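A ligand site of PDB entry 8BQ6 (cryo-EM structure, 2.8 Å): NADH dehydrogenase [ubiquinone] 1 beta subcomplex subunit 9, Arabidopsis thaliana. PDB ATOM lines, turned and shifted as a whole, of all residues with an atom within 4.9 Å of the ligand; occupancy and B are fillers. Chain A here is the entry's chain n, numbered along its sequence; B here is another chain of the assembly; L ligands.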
ATOM      1  N   ARG A  13     -34.422   7.742  23.971  1.00  0.00           N
ATOM      2  CA  ARG A  13     -33.144   8.115  24.577  1.00  0.00           C
ATOM      3  C   ARG A  13     -31.978   7.547  23.800  1.00  0.00           C
ATOM      4  O   ARG A  13     -30.971   8.244  23.635  1.00  0.00           O
ATOM      5  CB  ARG A  13     -33.091   7.684  26.042  1.00  0.00           C
ATOM      6  CG  ARG A  13     -33.956   8.524  26.941  1.00  0.00           C
ATOM      7  CD  ARG A  13     -33.252   9.800  27.396  1.00  0.00           C
ATOM      8  NE  ARG A  13     -31.985   9.537  28.087  1.00  0.00           N
ATOM      9  CZ  ARG A  13     -30.798   9.940  27.667  1.00  0.00           C
ATOM     10  NH1 ARG A  13     -30.662  10.675  26.571  1.00  0.00           N
ATOM     11  NH2 ARG A  13     -29.722   9.623  28.373  1.00  0.00           N
ATOM     12  N   LYS A  17     -28.792   9.216  22.164  1.00  0.00           N
ATOM     13  CA  LYS A  17     -27.413   8.788  22.362  1.00  0.00           C
ATOM     14  C   LYS A  17     -26.613   8.927  21.089  1.00  0.00           C
ATOM     15  O   LYS A  17     -25.483   9.433  21.101  1.00  0.00           O
ATOM     16  CB  LYS A  17     -27.374   7.341  22.856  1.00  0.00           C
ATOM     17  CG  LYS A  17     -28.056   7.140  24.166  1.00  0.00           C
ATOM     18  CD  LYS A  17     -27.330   7.794  25.278  1.00  0.00           C
ATOM     19  CE  LYS A  17     -28.079   7.543  26.547  1.00  0.00           C
ATOM     20  NZ  LYS A  17     -28.083   6.109  26.898  1.00  0.00           N
ATOM     21  N   VAL A  20     -25.432  12.506  20.184  1.00  0.00           N
ATOM     22  CA  VAL A  20     -24.287  12.977  20.957  1.00  0.00           C
ATOM     23  C   VAL A  20     -22.993  12.345  20.464  1.00  0.00           C
ATOM     24  O   VAL A  20     -21.978  13.018  20.299  1.00  0.00           O
ATOM     25  CB  VAL A  20     -24.510  12.692  22.456  1.00  0.00           C
ATOM     26  CG1 VAL A  20     -23.218  12.935  23.231  1.00  0.00           C
ATOM     27  CG2 VAL A  20     -25.626  13.559  23.004  1.00  0.00           C
ATOM     28  N   LEU A  23     -21.915  13.849  17.133  1.00  0.00           N
ATOM     29  CA  LEU A  23     -21.462  15.222  17.301  1.00  0.00           C
ATOM     30  C   LEU A  23     -20.094  15.270  17.959  1.00  0.00           C
ATOM     31  O   LEU A  23     -19.244  16.100  17.588  1.00  0.00           O
ATOM     32  CB  LEU A  23     -22.501  16.023  18.100  1.00  0.00           C
ATOM     33  CG  LEU A  23     -22.084  17.214  18.968  1.00  0.00           C
ATOM     34  CD1 LEU A  23     -21.515  18.348  18.133  1.00  0.00           C
ATOM     35  CD2 LEU A  23     -23.281  17.695  19.761  1.00  0.00           C
ATOM     36  N   ALA A  27     -17.063  16.972  16.096  1.00  0.00           N
ATOM     37  CA  ALA A  27     -16.371  18.064  16.765  1.00  0.00           C
ATOM     38  C   ALA A  27     -14.936  17.678  17.108  1.00  0.00           C
ATOM     39  O   ALA A  27     -14.063  18.550  17.206  1.00  0.00           O
ATOM     40  CB  ALA A  27     -17.137  18.468  18.025  1.00  0.00           C
ATOM     41  N   ASP A  30     -12.981  18.037  13.723  1.00  0.00           N
ATOM     42  CA  ASP A  30     -12.819  19.443  13.368  1.00  0.00           C
ATOM     43  C   ASP A  30     -11.861  20.153  14.302  1.00  0.00           C
ATOM     44  O   ASP A  30     -11.322  21.217  13.946  1.00  0.00           O
ATOM     45  CB  ASP A  30     -14.169  20.157  13.385  1.00  0.00           C
ATOM     46  CG  ASP A  30     -14.238  21.282  12.385  1.00  0.00           C
ATOM     47  OD1 ASP A  30     -13.810  21.079  11.231  1.00  0.00           O
ATOM     48  OD2 ASP A  30     -14.684  22.391  12.763  1.00  0.00           O
ATOM     49  N   LEU A  48     -12.378  19.658  24.716  1.00  0.00           N
ATOM     50  CA  LEU A  48     -13.662  19.352  24.101  1.00  0.00           C
ATOM     51  C   LEU A  48     -14.357  18.212  24.823  1.00  0.00           C
ATOM     52  O   LEU A  48     -15.589  18.216  24.962  1.00  0.00           O
ATOM     53  CB  LEU A  48     -13.456  19.017  22.625  1.00  0.00           C
ATOM     54  CG  LEU A  48     -14.737  18.969  21.781  1.00  0.00           C
ATOM     55  CD1 LEU A  48     -15.006  20.317  21.145  1.00  0.00           C
ATOM     56  CD2 LEU A  48     -14.608  17.873  20.735  1.00  0.00           C
ATOM     57  N   LYS A  51     -16.474  19.166  28.072  1.00  0.00           N
ATOM     58  CA  LYS A  51     -17.802  19.761  27.998  1.00  0.00           C
ATOM     59  C   LYS A  51     -18.846  18.659  27.903  1.00  0.00           C
ATOM     60  O   LYS A  51     -19.840  18.640  28.642  1.00  0.00           O
ATOM     61  CB  LYS A  51     -17.889  20.749  26.827  1.00  0.00           C
ATOM     62  CG  LYS A  51     -17.052  22.080  26.824  1.00  0.00           C
ATOM     63  CD  LYS A  51     -17.222  22.951  25.559  1.00  0.00           C
ATOM     64  CE  LYS A  51     -16.448  24.289  25.523  1.00  0.00           C
ATOM     65  NZ  LYS A  51     -16.448  25.198  24.486  1.00  0.00           N
ATOM     66  N   PHE A  52     -18.607  17.709  26.997  1.00  0.00           N
ATOM     67  CA  PHE A  52     -19.536  16.547  26.852  1.00  0.00           C
ATOM     68  C   PHE A  52     -19.705  15.856  28.211  1.00  0.00           C
ATOM     69  O   PHE A  52     -20.768  15.243  28.431  1.00  0.00           O
ATOM     70  CB  PHE A  52     -18.998  15.587  25.789  1.00  0.00           C
ATOM     71  CG  PHE A  52     -19.197  16.056  24.374  1.00  0.00           C
ATOM     72  CD1 PHE A  52     -20.382  15.809  23.689  1.00  0.00           C
ATOM     73  CD2 PHE A  52     -18.194  16.744  23.707  1.00  0.00           C
ATOM     74  CE1 PHE A  52     -20.563  16.250  22.389  1.00  0.00           C
ATOM     75  CE2 PHE A  52     -18.374  17.184  22.407  1.00  0.00           C
ATOM     76  CZ  PHE A  52     -19.551  16.935  21.750  1.00  0.00           C
ATOM     77  N   ASN A  55     -22.114  18.014  30.715  1.00  0.00           N
ATOM     78  CA  ASN A  55     -23.565  17.874  30.421  1.00  0.00           C
ATOM     79  C   ASN A  55     -24.006  16.398  30.480  1.00  0.00           C
ATOM     80  O   ASN A  55     -25.196  16.164  30.234  1.00  0.00           O
ATOM     81  CB  ASN A  55     -23.907  18.467  29.053  1.00  0.00           C
ATOM     82  CG  ASN A  55     -23.391  19.886  28.892  1.00  0.00           C
ATOM     83  OD1 ASN A  55     -22.492  20.129  28.087  1.00  0.00           O
ATOM     84  ND2 ASN A  55     -23.945  20.813  29.643  1.00  0.00           N
ATOM     85  N   GLN A  56     -23.108  15.463  30.813  1.00  0.00           N
ATOM     86  CA  GLN A  56     -23.461  14.013  30.779  1.00  0.00           C
ATOM     87  C   GLN A  56     -24.362  13.631  31.967  1.00  0.00           C
ATOM     88  O   GLN A  56     -24.960  12.524  31.908  1.00  0.00           O
ATOM     89  CB  GLN A  56     -22.175  13.170  30.713  1.00  0.00           C
ATOM     90  CG  GLN A  56     -21.261  13.289  31.926  1.00  0.00           C
ATOM     91  CD  GLN A  56     -20.018  12.435  31.775  1.00  0.00           C
ATOM     92  OE1 GLN A  56     -19.639  12.039  30.674  1.00  0.00           O
ATOM     93  NE2 GLN A  56     -19.386  12.133  32.895  1.00  0.00           N
ATOM     94  N   VAL A  58     -27.086  15.414  33.041  1.00  0.00           N
ATOM     95  CA  VAL A  58     -28.497  15.844  32.785  1.00  0.00           C
ATOM     96  C   VAL A  58     -29.372  14.623  32.492  1.00  0.00           C
ATOM     97  O   VAL A  58     -28.984  13.813  31.627  1.00  0.00           O
ATOM     98  CB  VAL A  58     -28.553  16.875  31.644  1.00  0.00           C
ATOM     99  CG1 VAL A  58     -29.971  17.400  31.403  1.00  0.00           C
ATOM    100  CG2 VAL A  58     -27.600  18.037  31.887  1.00  0.00           C
ATOM    101  N   ILE A  64     -31.977  17.723  27.466  1.00  0.00           N
ATOM    102  CA  ILE A  64     -30.934  17.052  26.637  1.00  0.00           C
ATOM    103  C   ILE A  64     -31.187  17.432  25.174  1.00  0.00           C
ATOM    104  O   ILE A  64     -30.242  17.887  24.525  1.00  0.00           O
ATOM    105  CB  ILE A  64     -30.973  15.535  26.865  1.00  0.00           C
ATOM    106  CG1 ILE A  64     -30.529  15.158  28.276  1.00  0.00           C
ATOM    107  CG2 ILE A  64     -30.160  14.783  25.807  1.00  0.00           C
ATOM    108  CD1 ILE A  64     -30.892  13.758  28.683  1.00  0.00           C
ATOM    109  N   LEU A  67     -29.737  20.659  24.779  1.00  0.00           N
ATOM    110  CA  LEU A  67     -28.289  20.700  24.713  1.00  0.00           C
ATOM    111  C   LEU A  67     -27.782  20.173  23.380  1.00  0.00           C
ATOM    112  O   LEU A  67     -26.844  20.721  22.797  1.00  0.00           O
ATOM    113  CB  LEU A  67     -27.673  19.915  25.871  1.00  0.00           C
ATOM    114  CG  LEU A  67     -27.848  20.498  27.273  1.00  0.00           C
ATOM    115  CD1 LEU A  67     -27.478  19.479  28.339  1.00  0.00           C
ATOM    116  CD2 LEU A  67     -26.989  21.740  27.423  1.00  0.00           C
ATOM    117  N   ILE A  68     -28.407  19.112  22.872  1.00  0.00           N
ATOM    118  CA  ILE A  68     -27.983  18.544  21.592  1.00  0.00           C
ATOM    119  C   ILE A  68     -28.151  19.556  20.476  1.00  0.00           C
ATOM    120  O   ILE A  68     -27.260  19.751  19.641  1.00  0.00           O
ATOM    121  CB  ILE A  68     -28.743  17.240  21.305  1.00  0.00           C
ATOM    122  CG1 ILE A  68     -28.135  16.068  22.072  1.00  0.00           C
ATOM    123  CG2 ILE A  68     -28.742  16.943  19.818  1.00  0.00           C
ATOM    124  CD1 ILE A  68     -28.970  14.825  22.037  1.00  0.00           C
ATOM    125  N   GLY A  71     -25.621  22.033  20.704  1.00  0.00           N
ATOM    126  CA  GLY A  71     -24.370  21.467  20.237  1.00  0.00           C
ATOM    127  C   GLY A  71     -24.228  21.517  18.727  1.00  0.00           C
ATOM    128  O   GLY A  71     -23.172  21.907  18.206  1.00  0.00           O
ATOM    129  N   GLU A  74     -23.498  25.012  17.588  1.00  0.00           N
ATOM    130  CA  GLU A  74     -22.109  25.391  17.839  1.00  0.00           C
ATOM    131  C   GLU A  74     -21.174  24.770  16.823  1.00  0.00           C
ATOM    132  O   GLU A  74     -20.239  25.425  16.341  1.00  0.00           O
ATOM    133  CB  GLU A  74     -21.724  24.990  19.263  1.00  0.00           C
ATOM    134  CG  GLU A  74     -22.439  25.808  20.314  1.00  0.00           C
ATOM    135  CD  GLU A  74     -22.512  27.273  19.954  1.00  0.00           C
ATOM    136  OE1 GLU A  74     -21.513  27.990  20.207  1.00  0.00           O
ATOM    137  OE2 GLU A  74     -23.541  27.706  19.413  1.00  0.00           O
ATOM    138  N   TYR A  75     -21.389  23.500  16.490  1.00  0.00           N
ATOM    139  CA  TYR A  75     -20.545  22.841  15.498  1.00  0.00           C
ATOM    140  C   TYR A  75     -20.717  23.484  14.123  1.00  0.00           C
ATOM    141  O   TYR A  75     -19.736  23.729  13.426  1.00  0.00           O
ATOM    142  CB  TYR A  75     -20.863  21.348  15.439  1.00  0.00           C
ATOM    143  CG  TYR A  75     -20.204  20.654  14.265  1.00  0.00           C
ATOM    144  CD1 TYR A  75     -18.857  20.346  14.289  1.00  0.00           C
ATOM    145  CD2 TYR A  75     -20.941  20.335  13.135  1.00  0.00           C
ATOM    146  CE1 TYR A  75     -18.256  19.720  13.205  1.00  0.00           C
ATOM    147  CE2 TYR A  75     -20.348  19.711  12.057  1.00  0.00           C
ATOM    148  CZ  TYR A  75     -19.011  19.412  12.099  1.00  0.00           C
ATOM    149  OH  TYR A  75     -18.426  18.789  11.010  1.00  0.00           O
ATOM    150  N   TRP A  78     -18.919  27.177  14.346  1.00  0.00           N
ATOM    151  CA  TRP A  78     -17.470  27.227  14.493  1.00  0.00           C
ATOM    152  C   TRP A  78     -16.758  26.150  13.689  1.00  0.00           C
ATOM    153  O   TRP A  78     -15.611  25.805  14.010  1.00  0.00           O
ATOM    154  CB  TRP A  78     -17.079  27.113  15.966  1.00  0.00           C
ATOM    155  CG  TRP A  78     -17.736  28.133  16.825  1.00  0.00           C
ATOM    156  CD1 TRP A  78     -18.771  27.946  17.687  1.00  0.00           C
ATOM    157  CD2 TRP A  78     -17.385  29.523  16.922  1.00  0.00           C
ATOM    158  NE1 TRP A  78     -19.094  29.124  18.307  1.00  0.00           N
ATOM    159  CE2 TRP A  78     -18.264  30.105  17.854  1.00  0.00           C
ATOM    160  CE3 TRP A  78     -16.417  30.327  16.310  1.00  0.00           C
ATOM    161  CZ2 TRP A  78     -18.202  31.459  18.181  1.00  0.00           C
ATOM    162  CZ3 TRP A  78     -16.359  31.667  16.637  1.00  0.00           C
ATOM    163  CH2 TRP A  78     -17.244  32.221  17.569  1.00  0.00           C
ATOM    164  N   ARG A  79     -17.418  25.595  12.671  1.00  0.00           N
ATOM    165  CA  ARG A  79     -16.828  24.552  11.847  1.00  0.00           C
ATOM    166  C   ARG A  79     -15.676  25.118  11.022  1.00  0.00           C
ATOM    167  O   ARG A  79     -15.668  26.283  10.646  1.00  0.00           O
ATOM    168  CB  ARG A  79     -17.907  23.963  10.924  1.00  0.00           C
ATOM    169  CG  ARG A  79     -17.572  22.655  10.219  1.00  0.00           C
ATOM    170  CD  ARG A  79     -18.155  22.606   8.804  1.00  0.00           C
ATOM    171  NE  ARG A  79     -18.852  21.360   8.518  1.00  0.00           N
ATOM    172  CZ  ARG A  79     -18.288  20.273   8.005  1.00  0.00           C
ATOM    173  NH1 ARG A  79     -16.999  20.245   7.698  1.00  0.00           N
ATOM    174  NH2 ARG A  79     -19.030  19.194   7.800  1.00  0.00           N
ATOM    175  N   GLN B  72     -17.581  -1.195  25.681  1.00  0.00           N
ATOM    176  CA  GLN B  72     -18.417  -0.693  26.807  1.00  0.00           C
ATOM    177  C   GLN B  72     -18.742  -1.791  27.834  1.00  0.00           C
ATOM    178  O   GLN B  72     -19.099  -1.414  28.968  1.00  0.00           O
ATOM    179  CB  GLN B  72     -19.712  -0.079  26.271  1.00  0.00           C
ATOM    180  CG  GLN B  72     -19.508   1.275  25.619  1.00  0.00           C
ATOM    181  CD  GLN B  72     -20.714   1.716  24.827  1.00  0.00           C
ATOM    182  OE1 GLN B  72     -21.639   2.332  25.357  1.00  0.00           O
ATOM    183  NE2 GLN B  72     -20.715   1.386  23.546  1.00  0.00           N
ATOM    184  N   ASP B  78     -16.896   4.212  28.516  1.00  0.00           N
ATOM    185  CA  ASP B  78     -18.066   4.948  28.062  1.00  0.00           C
ATOM    186  C   ASP B  78     -18.101   4.993  26.539  1.00  0.00           C
ATOM    187  O   ASP B  78     -17.110   4.721  25.855  1.00  0.00           O
ATOM    188  CB  ASP B  78     -18.065   6.360  28.629  1.00  0.00           C
ATOM    189  CG  ASP B  78     -17.456   6.418  30.009  1.00  0.00           C
ATOM    190  OD1 ASP B  78     -16.404   7.061  30.183  1.00  0.00           O
ATOM    191  OD2 ASP B  78     -18.048   5.801  30.929  1.00  0.00           O
ATOM    192  N   SER B  79     -19.274   5.319  26.003  1.00  0.00           N
ATOM    193  CA  SER B  79     -19.411   5.406  24.553  1.00  0.00           C
ATOM    194  C   SER B  79     -18.543   6.498  23.953  1.00  0.00           C
ATOM    195  O   SER B  79     -18.033   6.320  22.849  1.00  0.00           O
ATOM    196  CB  SER B  79     -20.851   5.621  24.165  1.00  0.00           C
ATOM    197  OG  SER B  79     -21.193   6.996  24.259  1.00  0.00           O
ATOM    198  N   LEU B  80     -18.385   7.634  24.647  1.00  0.00           N
ATOM    199  CA  LEU B  80     -17.454   8.624  24.140  1.00  0.00           C
ATOM    200  C   LEU B  80     -16.058   8.040  24.033  1.00  0.00           C
ATOM    201  O   LEU B  80     -15.359   8.295  23.048  1.00  0.00           O
ATOM    202  CB  LEU B  80     -17.441   9.874  25.014  1.00  0.00           C
ATOM    203  CG  LEU B  80     -18.760  10.597  25.250  1.00  0.00           C
ATOM    204  CD1 LEU B  80     -18.496  11.913  25.936  1.00  0.00           C
ATOM    205  CD2 LEU B  80     -19.508  10.813  23.951  1.00  0.00           C
HETATM  206  O1  LIG L   1     -24.269  19.654  25.439  1.00  0.00           O
HETATM  207  C1  LIG L   1     -16.429  22.875  15.937  1.00  0.00           C
HETATM  208  O2  LIG L   1     -20.362   7.994  26.984  1.00  0.00           O
HETATM  209  C2  LIG L   1     -16.924  22.436  17.287  1.00  0.00           C
HETATM  210  C3  LIG L   1     -17.643  23.508  18.051  1.00  0.00           C
HETATM  211  C4  LIG L   1     -18.177  23.078  19.397  1.00  0.00           C
HETATM  212  O3  LIG L   1     -21.902   6.079  27.553  1.00  0.00           O
HETATM  213  C5  LIG L   1     -19.073  21.862  19.359  1.00  0.00           C
HETATM  214  C6  LIG L   1     -19.138  21.099  20.655  1.00  0.00           C
HETATM  215  C7  LIG L   1     -20.536  20.799  21.123  1.00  0.00           C
HETATM  216  C8  LIG L   1     -20.845  21.223  22.541  1.00  0.00           C
HETATM  217  C9  LIG L   1     -20.416  20.228  23.594  1.00  0.00           C
HETATM  218  C10 LIG L   1     -21.529  19.753  24.495  1.00  0.00           C
HETATM  219  C11 LIG L   1     -22.664  19.113  23.763  1.00  0.00           C
HETATM  220  C12 LIG L   1     -23.906  18.901  24.577  1.00  0.00           C
HETATM  221  C13 LIG L   1     -22.568   9.722  26.600  1.00  0.00           C
HETATM  222  C14 LIG L   1     -23.814  10.565  26.885  1.00  0.00           C
HETATM  223  C15 LIG L   1     -23.374  12.023  26.981  1.00  0.00           C
HETATM  224  C16 LIG L   1     -24.768  10.411  25.694  1.00  0.00           C
HETATM  225  C17 LIG L   1     -24.497  10.111  28.193  1.00  0.00           C
HETATM  226  C18 LIG L   1     -25.980  10.436  28.404  1.00  0.00           C
HETATM  227  C19 LIG L   1     -26.941  12.567  29.158  1.00  0.00           C
HETATM  228  C20 LIG L   1     -27.050  14.000  28.659  1.00  0.00           C
HETATM  229  C21 LIG L   1     -26.340  14.304  27.358  1.00  0.00           C
HETATM  230  C22 LIG L   1     -24.632  15.717  26.274  1.00  0.00           C
HETATM  231  C23 LIG L   1     -25.394  16.895  25.737  1.00  0.00           C
HETATM  232  N1  LIG L   1     -26.406  11.664  28.143  1.00  0.00           N
HETATM  233  N2  LIG L   1     -25.285  15.115  27.427  1.00  0.00           N
HETATM  234  O4  LIG L   1     -22.813   8.346  27.022  1.00  0.00           O
HETATM  235  O5  LIG L   1     -23.751  10.609  29.288  1.00  0.00           O
HETATM  236  O6  LIG L   1     -26.720   9.565  28.846  1.00  0.00           O
HETATM  237  O7  LIG L   1     -26.735  13.822  26.301  1.00  0.00           O
HETATM  238  P1  LIG L   1     -21.601   7.558  27.728  1.00  0.00           P
HETATM  239  S1  LIG L   1     -24.783  17.445  24.127  1.00  0.00           S
HETATM  240  O8  LIG L   1     -21.615   7.989  29.180  1.00  0.00           O
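N2 of the ligand is in hydrogen-bond range of O of Asn 55.
The side-chain amide oxygen of Asn 55 sits close to an oxygen (O1) of the ligand, at 3.2 Å.
O2 of the ligand is in hydrogen-bond range of N of Ser 79 of chain B (3.0 Å).
OG of Ser 79 of chain B is in hydrogen-bond range of O2 of the ligand (3.0 Å).
The guanidinium group (NH2) of Arg 13 is in hydrogen-bond range of an oxygen (O6) of the ligand (3.0 Å).
The backbone NH (N) of Leu 80 of chain B sits at hydrogen-bond distance from an oxygen (O2) of the ligand, at 3.1 Å.
An oxygen (O5) of the ligand sits close to the backbone carbonyl oxygen of Gln 56 (3.5 Å).
O of Lys 51 lies close to OD1 of Asn 55.
The side-chain carboxylate of Glu 74 sits at hydrogen-bond distance from the indole nitrogen of Trp 78 of chain A (3.3 Å).
The side-chain hydroxyl (OH) of Tyr 75 is in hydrogen-bond range of the guanidinium group (NH2) of Arg 79 of chain A (3.3 Å).
CE of Lys 17 touches O6 of the ligand (3.3 Å).
CG2 of Val 20 touches O7 of the ligand, 3.5 Å away.
CD1 of Leu 23 touches C7 of the ligand, at 3.99 Å.
Asp 30 touches the ligand.
CE1 of Phe 52 touches C11 of the ligand (3.8 Å).
O of Val 58 touches C19 of the ligand, 3.4 Å away.
CG2 of Ile 64 touches O7 of the ligand (3.6 Å).
Leu 67 touches the ligand (CB to O1, 3.4 Å).
CA of Gly 71 touches C7 of the ligand, at 3.99 Å.
O of Glu 74 touches C3 of the ligand (3.7 Å).
CD1 of Tyr 75 touches C1 of the ligand, at 3.9 Å.
O of Trp 78 of chain A touches C1 of the ligand, 3.6 Å away.
Asp 78 of chain B touches the ligand (CB to O2, 3.3 Å).
Hydrophobic or aromatic side chains within 4 Å of the ligand: Val 20, Leu 23, Phe 52, Ile 64, Leu 67, Tyr 75 and Leu 80 of chain B.
Within 4 Å of the ligand: Arg 13, Lys 17, Val 20, Leu 23, Asp 30, Phe 52, Asn 55, Gln 56, Val 58, Ile 64, Leu 67, Gly 71, Glu 74, Tyr 75, Trp 78 of chain A, Asp 78 of chain B, Ser 79 of chain B and Leu 80 of chain B.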
